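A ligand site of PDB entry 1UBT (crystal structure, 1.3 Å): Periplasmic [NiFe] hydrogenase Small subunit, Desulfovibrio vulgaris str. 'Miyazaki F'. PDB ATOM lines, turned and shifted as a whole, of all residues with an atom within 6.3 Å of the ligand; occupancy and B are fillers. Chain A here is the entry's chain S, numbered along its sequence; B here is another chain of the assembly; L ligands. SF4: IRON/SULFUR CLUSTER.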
ATOM      1  N   ALA A  15      -8.788 -11.894  24.480  1.00  0.00           N
ATOM      2  CA  ALA A  15      -9.151 -13.140  23.807  1.00  0.00           C
ATOM      3  C   ALA A  15      -8.762 -14.250  24.778  1.00  0.00           C
ATOM      4  O   ALA A  15      -7.607 -14.592  24.925  1.00  0.00           O
ATOM      5  CB  ALA A  15      -8.467 -13.286  22.459  1.00  0.00           C
ATOM      6  N   GLU A  16      -9.790 -14.801  25.443  1.00  0.00           N
ATOM      7  CA  GLU A  16      -9.575 -15.657  26.596  1.00  0.00           C
ATOM      8  C   GLU A  16     -10.735 -16.630  26.710  1.00  0.00           C
ATOM      9  O   GLU A  16     -11.766 -16.459  26.090  1.00  0.00           O
ATOM     10  CB  GLU A  16      -9.391 -14.858  27.899  1.00  0.00           C
ATOM     11  CG  GLU A  16     -10.385 -13.714  28.102  1.00  0.00           C
ATOM     12  CD  GLU A  16     -11.749 -14.086  28.660  1.00  0.00           C
ATOM     13  OE1 GLU A  16     -11.805 -14.965  29.555  1.00  0.00           O
ATOM     14  OE2 GLU A  16     -12.767 -13.469  28.218  1.00  0.00           O
ATOM     15  N   CYS A  17     -10.525 -17.698  27.483  1.00  0.00           N
ATOM     16  CA  CYS A  17     -11.516 -18.722  27.694  1.00  0.00           C
ATOM     17  C   CYS A  17     -12.127 -18.658  29.100  1.00  0.00           C
ATOM     18  O   CYS A  17     -13.013 -19.443  29.421  1.00  0.00           O
ATOM     19  CB  CYS A  17     -10.914 -20.117  27.507  1.00  0.00           C
ATOM     20  SG  CYS A  17      -9.941 -20.745  28.923  1.00  0.00           S
ATOM     21  N   THR A  18     -11.629 -17.743  29.924  1.00  0.00           N
ATOM     22  CA  THR A  18     -12.090 -17.465  31.292  1.00  0.00           C
ATOM     23  C   THR A  18     -11.572 -18.522  32.267  1.00  0.00           C
ATOM     24  O   THR A  18     -11.856 -18.459  33.457  1.00  0.00           O
ATOM     25  CB  THR A  18     -13.604 -17.226  31.323  1.00  0.00           C
ATOM     26  OG1 THR A  18     -13.923 -16.311  30.241  1.00  0.00           O
ATOM     27  CG2 THR A  18     -14.054 -16.559  32.624  1.00  0.00           C
ATOM     28  N   GLY A  19     -10.735 -19.466  31.798  1.00  0.00           N
ATOM     29  CA  GLY A  19     -10.071 -20.411  32.688  1.00  0.00           C
ATOM     30  C   GLY A  19      -9.120 -19.697  33.627  1.00  0.00           C
ATOM     31  O   GLY A  19      -8.943 -20.148  34.798  1.00  0.00           O
ATOM     32  N   CYS A  20      -8.486 -18.610  33.178  1.00  0.00           N
ATOM     33  CA  CYS A  20      -7.611 -17.930  34.124  1.00  0.00           C
ATOM     34  C   CYS A  20      -8.418 -17.251  35.216  1.00  0.00           C
ATOM     35  O   CYS A  20      -8.084 -17.290  36.417  1.00  0.00           O
ATOM     36  CB  CYS A  20      -6.693 -16.938  33.358  1.00  0.00           C
ATOM     37  SG  CYS A  20      -5.407 -17.746  32.418  1.00  0.00           S
ATOM     38  N   SER A  21      -9.535 -16.594  34.876  1.00  0.00           N
ATOM     39  CA  SER A  21     -10.394 -16.048  35.921  1.00  0.00           C
ATOM     40  C   SER A  21     -10.865 -17.137  36.869  1.00  0.00           C
ATOM     41  O   SER A  21     -10.886 -16.908  38.076  1.00  0.00           O
ATOM     42  CB  SER A  21     -11.671 -15.414  35.324  1.00  0.00           C
ATOM     43  OG  SER A  21     -11.387 -14.168  34.764  1.00  0.00           O
ATOM     44  N   GLU A  75      -6.086 -10.890  31.356  1.00  0.00           N
ATOM     45  CA  GLU A  75      -6.300 -12.286  30.889  1.00  0.00           C
ATOM     46  C   GLU A  75      -6.584 -12.266  29.390  1.00  0.00           C
ATOM     47  O   GLU A  75      -7.388 -11.416  28.949  1.00  0.00           O
ATOM     48  CB  GLU A  75      -7.458 -12.903  31.687  1.00  0.00           C
ATOM     49  CG  GLU A  75      -7.942 -14.286  31.271  1.00  0.00           C
ATOM     50  CD  GLU A  75      -9.056 -14.837  32.161  1.00  0.00           C
ATOM     51  OE1 GLU A  75      -9.484 -15.990  31.908  1.00  0.00           O
ATOM     52  OE2 GLU A  75      -9.442 -14.067  33.082  1.00  0.00           O
ATOM     53  N   GLY A  76      -5.942 -13.138  28.630  1.00  0.00           N
ATOM     54  CA  GLY A  76      -6.224 -13.292  27.216  1.00  0.00           C
ATOM     55  C   GLY A  76      -5.210 -12.546  26.337  1.00  0.00           C
ATOM     56  O   GLY A  76      -4.607 -11.529  26.720  1.00  0.00           O
ATOM     57  N   GLY A  77      -5.066 -13.088  25.127  1.00  0.00           N
ATOM     58  CA  GLY A  77      -4.291 -12.497  24.071  1.00  0.00           C
ATOM     59  C   GLY A  77      -4.968 -11.283  23.452  1.00  0.00           C
ATOM     60  O   GLY A  77      -6.177 -11.142  23.565  1.00  0.00           O
ATOM     61  N   TYR A 111      -1.699 -12.484  33.061  1.00  0.00           N
ATOM     62  CA  TYR A 111      -2.029 -13.702  33.793  1.00  0.00           C
ATOM     63  C   TYR A 111      -2.575 -14.722  32.803  1.00  0.00           C
ATOM     64  O   TYR A 111      -3.607 -14.507  32.175  1.00  0.00           O
ATOM     65  CB  TYR A 111      -3.035 -13.390  34.908  1.00  0.00           C
ATOM     66  CG  TYR A 111      -3.329 -14.609  35.776  1.00  0.00           C
ATOM     67  CD1 TYR A 111      -2.309 -15.228  36.514  1.00  0.00           C
ATOM     68  CD2 TYR A 111      -4.609 -15.115  35.839  1.00  0.00           C
ATOM     69  CE1 TYR A 111      -2.541 -16.330  37.313  1.00  0.00           C
ATOM     70  CE2 TYR A 111      -4.855 -16.240  36.611  1.00  0.00           C
ATOM     71  CZ  TYR A 111      -3.839 -16.852  37.361  1.00  0.00           C
ATOM     72  OH  TYR A 111      -4.058 -17.955  38.131  1.00  0.00           O
ATOM     73  N   GLY A 112      -1.797 -15.809  32.646  1.00  0.00           N
ATOM     74  CA  GLY A 112      -2.030 -16.906  31.773  1.00  0.00           C
ATOM     75  C   GLY A 112      -1.241 -16.811  30.466  1.00  0.00           C
ATOM     76  O   GLY A 112      -0.925 -15.703  30.008  1.00  0.00           O
ATOM     77  N   THR A 113      -0.920 -17.974  29.911  1.00  0.00           N
ATOM     78  CA  THR A 113      -0.117 -18.024  28.694  1.00  0.00           C
ATOM     79  C   THR A 113      -0.722 -17.203  27.571  1.00  0.00           C
ATOM     80  O   THR A 113       0.044 -16.715  26.735  1.00  0.00           O
ATOM     81  CB  THR A 113       0.035 -19.531  28.290  1.00  0.00           C
ATOM     82  OG1 THR A 113       0.821 -20.076  29.376  1.00  0.00           O
ATOM     83  CG2 THR A 113       0.759 -19.724  26.960  1.00  0.00           C
ATOM     84  N   CYS A 114      -2.019 -17.067  27.471  1.00  0.00           N
ATOM     85  CA  CYS A 114      -2.544 -16.201  26.405  1.00  0.00           C
ATOM     86  C   CYS A 114      -2.100 -14.756  26.598  1.00  0.00           C
ATOM     87  O   CYS A 114      -1.599 -14.121  25.658  1.00  0.00           O
ATOM     88  CB  CYS A 114      -4.069 -16.199  26.388  1.00  0.00           C
ATOM     89  SG  CYS A 114      -4.823 -17.823  25.925  1.00  0.00           S
ATOM     90  N   ALA A 115      -2.311 -14.214  27.807  1.00  0.00           N
ATOM     91  CA  ALA A 115      -1.854 -12.839  28.019  1.00  0.00           C
ATOM     92  C   ALA A 115      -0.343 -12.736  28.005  1.00  0.00           C
ATOM     93  O   ALA A 115       0.228 -11.705  27.597  1.00  0.00           O
ATOM     94  CB  ALA A 115      -2.392 -12.323  29.364  1.00  0.00           C
ATOM     95  N   GLY A 119      -0.832 -17.467  23.419  1.00  0.00           N
ATOM     96  CA  GLY A 119      -1.711 -18.564  23.794  1.00  0.00           C
ATOM     97  C   GLY A 119      -2.474 -19.216  22.669  1.00  0.00           C
ATOM     98  O   GLY A 119      -2.043 -19.198  21.524  1.00  0.00           O
ATOM     99  N   VAL A 120      -3.638 -19.817  22.998  1.00  0.00           N
ATOM    100  CA  VAL A 120      -4.230 -20.800  22.090  1.00  0.00           C
ATOM    101  C   VAL A 120      -4.648 -20.150  20.785  1.00  0.00           C
ATOM    102  O   VAL A 120      -4.473 -20.709  19.693  1.00  0.00           O
ATOM    103  CB  VAL A 120      -5.404 -21.546  22.766  1.00  0.00           C
ATOM    104  CG1 VAL A 120      -6.606 -20.659  23.046  1.00  0.00           C
ATOM    105  CG2 VAL A 120      -5.770 -22.768  21.922  1.00  0.00           C
ATOM    106  N   GLN A 121      -5.190 -18.926  20.819  1.00  0.00           N
ATOM    107  CA  GLN A 121      -5.622 -18.300  19.558  1.00  0.00           C
ATOM    108  C   GLN A 121      -4.437 -17.812  18.733  1.00  0.00           C
ATOM    109  O   GLN A 121      -4.594 -17.512  17.546  1.00  0.00           O
ATOM    110  CB  GLN A 121      -6.643 -17.147  19.798  1.00  0.00           C
ATOM    111  CG  GLN A 121      -6.151 -16.040  20.741  1.00  0.00           C
ATOM    112  CD  GLN A 121      -6.339 -16.404  22.183  1.00  0.00           C
ATOM    113  OE1 GLN A 121      -7.420 -16.909  22.576  1.00  0.00           O
ATOM    114  NE2 GLN A 121      -5.362 -16.219  23.068  1.00  0.00           N
ATOM    115  N   GLY A 149       1.022 -20.242  32.232  1.00  0.00           N
ATOM    116  CA  GLY A 149       0.301 -21.470  32.495  1.00  0.00           C
ATOM    117  C   GLY A 149      -1.088 -21.343  31.837  1.00  0.00           C
ATOM    118  O   GLY A 149      -1.596 -20.210  31.634  1.00  0.00           O
ATOM    119  N   CYS A 150      -1.731 -22.493  31.636  1.00  0.00           N
ATOM    120  CA  CYS A 150      -2.997 -22.486  30.897  1.00  0.00           C
ATOM    121  C   CYS A 150      -4.045 -23.317  31.612  1.00  0.00           C
ATOM    122  O   CYS A 150      -4.437 -24.398  31.143  1.00  0.00           O
ATOM    123  CB  CYS A 150      -2.699 -23.016  29.490  1.00  0.00           C
ATOM    124  SG  CYS A 150      -4.028 -22.734  28.290  1.00  0.00           S
ATOM    125  N   PRO A 151      -4.591 -22.833  32.731  1.00  0.00           N
ATOM    126  CA  PRO A 151      -4.211 -21.582  33.392  1.00  0.00           C
ATOM    127  C   PRO A 151      -3.070 -21.738  34.393  1.00  0.00           C
ATOM    128  O   PRO A 151      -2.652 -22.859  34.717  1.00  0.00           O
ATOM    129  CB  PRO A 151      -5.479 -21.222  34.158  1.00  0.00           C
ATOM    130  CG  PRO A 151      -6.016 -22.605  34.550  1.00  0.00           C
ATOM    131  CD  PRO A 151      -5.743 -23.526  33.378  1.00  0.00           C
ATOM    132  N   PRO A 152      -2.540 -20.608  34.845  1.00  0.00           N
ATOM    133  CA  PRO A 152      -1.472 -20.639  35.849  1.00  0.00           C
ATOM    134  C   PRO A 152      -1.975 -21.206  37.163  1.00  0.00           C
ATOM    135  O   PRO A 152      -3.179 -21.251  37.394  1.00  0.00           O
ATOM    136  CB  PRO A 152      -1.050 -19.172  36.071  1.00  0.00           C
ATOM    137  CG  PRO A 152      -1.595 -18.481  34.831  1.00  0.00           C
ATOM    138  CD  PRO A 152      -2.898 -19.214  34.525  1.00  0.00           C
ATOM    139  N   TRP A 258       1.581 -24.417  22.033  1.00  0.00           N
ATOM    140  CA  TRP A 258       0.643 -25.131  21.160  1.00  0.00           C
ATOM    141  C   TRP A 258       1.347 -25.594  19.884  1.00  0.00           C
ATOM    142  O   TRP A 258       0.924 -26.611  19.313  1.00  0.00           O
ATOM    143  CB  TRP A 258      -0.502 -24.201  20.753  1.00  0.00           C
ATOM    144  CG  TRP A 258      -1.250 -23.753  21.978  1.00  0.00           C
ATOM    145  CD1 TRP A 258      -1.178 -22.547  22.637  1.00  0.00           C
ATOM    146  CD2 TRP A 258      -2.178 -24.546  22.710  1.00  0.00           C
ATOM    147  NE1 TRP A 258      -2.024 -22.548  23.720  1.00  0.00           N
ATOM    148  CE2 TRP A 258      -2.655 -23.767  23.798  1.00  0.00           C
ATOM    149  CE3 TRP A 258      -2.650 -25.854  22.548  1.00  0.00           C
ATOM    150  CZ2 TRP A 258      -3.604 -24.249  24.739  1.00  0.00           C
ATOM    151  CZ3 TRP A 258      -3.590 -26.349  23.466  1.00  0.00           C
ATOM    152  CH2 TRP A 258      -4.040 -25.552  24.527  1.00  0.00           C
ATOM    153  N   ARG B  41     -11.918 -16.348  18.021  1.00  0.00           N
ATOM    154  CA  ARG B  41     -10.603 -16.937  18.158  1.00  0.00           C
ATOM    155  C   ARG B  41     -10.268 -17.851  16.998  1.00  0.00           C
ATOM    156  O   ARG B  41      -9.094 -17.826  16.567  1.00  0.00           O
ATOM    157  CB  ARG B  41     -10.475 -17.667  19.506  1.00  0.00           C
ATOM    158  CG  ARG B  41     -10.368 -16.679  20.677  1.00  0.00           C
ATOM    159  CD  ARG B  41     -10.379 -17.282  22.052  1.00  0.00           C
ATOM    160  NE  ARG B  41     -11.595 -18.048  22.205  1.00  0.00           N
ATOM    161  CZ  ARG B  41     -11.783 -19.117  22.967  1.00  0.00           C
ATOM    162  NH1 ARG B  41     -10.827 -19.578  23.770  1.00  0.00           N
ATOM    163  NH2 ARG B  41     -12.959 -19.756  22.959  1.00  0.00           N
ATOM    164  N   ARG B  61      -9.606 -25.489  25.666  1.00  0.00           N
ATOM    165  CA  ARG B  61      -9.435 -24.040  25.868  1.00  0.00           C
ATOM    166  C   ARG B  61     -10.488 -23.238  25.114  1.00  0.00           C
ATOM    167  O   ARG B  61     -10.412 -22.017  25.049  1.00  0.00           O
ATOM    168  CB  ARG B  61      -8.036 -23.595  25.447  1.00  0.00           C
ATOM    169  CG  ARG B  61      -6.993 -23.873  26.497  1.00  0.00           C
ATOM    170  CD  ARG B  61      -6.817 -25.366  26.794  1.00  0.00           C
ATOM    171  NE  ARG B  61      -5.780 -25.465  27.842  1.00  0.00           N
ATOM    172  CZ  ARG B  61      -5.340 -26.621  28.342  1.00  0.00           C
ATOM    173  NH1 ARG B  61      -5.820 -27.773  27.827  1.00  0.00           N
ATOM    174  NH2 ARG B  61      -4.464 -26.649  29.328  1.00  0.00           N
ATOM    175  N   GLY B  64     -13.003 -22.160  29.923  1.00  0.00           N
ATOM    176  CA  GLY B  64     -12.560 -22.536  31.259  1.00  0.00           C
ATOM    177  C   GLY B  64     -13.617 -22.465  32.337  1.00  0.00           C
ATOM    178  O   GLY B  64     -13.339 -22.826  33.462  1.00  0.00           O
ATOM    179  N   PRO B 216      -8.910 -25.237  36.877  1.00  0.00           N
ATOM    180  CA  PRO B 216      -9.442 -25.570  35.555  1.00  0.00           C
ATOM    181  C   PRO B 216      -8.492 -26.359  34.643  1.00  0.00           C
ATOM    182  O   PRO B 216      -7.245 -26.367  34.865  1.00  0.00           O
ATOM    183  CB  PRO B 216      -9.637 -24.162  34.901  1.00  0.00           C
ATOM    184  CG  PRO B 216      -9.736 -23.207  36.071  1.00  0.00           C
ATOM    185  CD  PRO B 216      -8.694 -23.782  37.034  1.00  0.00           C
ATOM    186  N   HIS B 217      -9.121 -26.938  33.589  1.00  0.00           N
ATOM    187  CA  HIS B 217      -8.542 -27.611  32.437  1.00  0.00           C
ATOM    188  C   HIS B 217      -7.913 -28.919  32.894  1.00  0.00           C
ATOM    189  O   HIS B 217      -6.746 -29.066  33.216  1.00  0.00           O
ATOM    190  CB  HIS B 217      -7.544 -26.706  31.685  1.00  0.00           C
ATOM    191  CG  HIS B 217      -8.308 -25.626  30.928  1.00  0.00           C
ATOM    192  ND1 HIS B 217      -7.813 -24.480  30.388  1.00  0.00           N
ATOM    193  CD2 HIS B 217      -9.675 -25.676  30.682  1.00  0.00           C
ATOM    194  CE1 HIS B 217      -8.844 -23.816  29.802  1.00  0.00           C
ATOM    195  NE2 HIS B 217      -9.935 -24.548  29.985  1.00  0.00           N
HETATM  196 FE1  SF4 L   1      -7.805 -19.917  28.830  1.00  0.00          FE
HETATM  197 FE2  SF4 L   1      -5.744 -18.590  27.813  1.00  0.00          FE
HETATM  198 FE3  SF4 L   1      -5.338 -20.945  28.927  1.00  0.00          FE
HETATM  199 FE4  SF4 L   1      -5.997 -18.839  30.520  1.00  0.00          FE
HETATM  200  S1  SF4 L   1      -4.057 -19.056  29.331  1.00  0.00           S
HETATM  201  S2  SF4 L   1      -6.773 -20.971  30.621  1.00  0.00           S
HETATM  202  S3  SF4 L   1      -7.395 -17.642  29.089  1.00  0.00           S
HETATM  203  S4  SF4 L   1      -6.628 -20.545  27.008  1.00  0.00           S
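A ring nitrogen (ND1) of His 217 of chain B lies close to a sulfur (S2) of the ligand.
A sulfur (S1) of the ligand lies close to the backbone NH (N) of Cys 114 (3.4 Å).
The side-chain sulfur (SG) of Cys 150 binds an iron atom (FE3) of the ligand (2.3 Å).
FE1 of the ligand is bound by SG of Cys 17 (2.3 Å).
The backbone NH (N) of Thr 113 sits close to a sulfur (S1) of the ligand (3.4 Å).
An iron atom (FE2) of the ligand is bound by the side-chain sulfur (SG) of Cys 114 (2.2 Å).
The backbone NH (N) of Cys 17 sits close to a sulfur (S3) of the ligand.
The side-chain sulfur of Cys 20 binds an iron atom (FE4) of the ligand, at 2.3 Å.
The side-chain hydroxyl of Thr 18 sits at hydrogen-bond distance from the side-chain carboxylate of Glu 16 (2.6 Å).
The side-chain sulfur (SG) of Cys 20 lies close to the backbone carbonyl oxygen (O) of Tyr 111 (3.7 Å).
SG of Cys 114 sits close to NE2 of Gln 121, 3.3 Å away.
N of Gly 19 lies close to SG of Cys 17 (3.2 Å).
OE1 of Glu 75 lies close to N of Thr 18, 3.4 Å away.
O of Cys 150 sits at hydrogen-bond distance from ND1 of His 217 of chain B (3.5 Å).
The side-chain sulfur (SG) of Cys 114 sits close to the backbone NH (N) of Val 120 (3.7 Å).
OG1 of Thr 113 lies within hydrogen-bond range of N of Gly 149, at 2.9 Å.
A sulfur (S1) of the ligand sits close to the backbone carbonyl oxygen of Gly 149, 3.6 Å away.
The backbone nitrogen (N) of Pro 151 sits close to a sulfur (S2) of the ligand (3.6 Å).
Residues that only touch the ligand: Arg 61 of chain B (3.4 Å), Glu 16 (3.6 Å), Gly 112 (3.8 Å), Glu 75 (3.9 Å), Gly 19 (3.9 Å) and Val 120 (3.96 Å).
Hydrophobic or aromatic side chains within 4 Å of the ligand: Val 120, Pro 151 and His 217 of chain B.
The nearest printed residue that does not touch the ligand is Thr 18 (4.3 Å).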
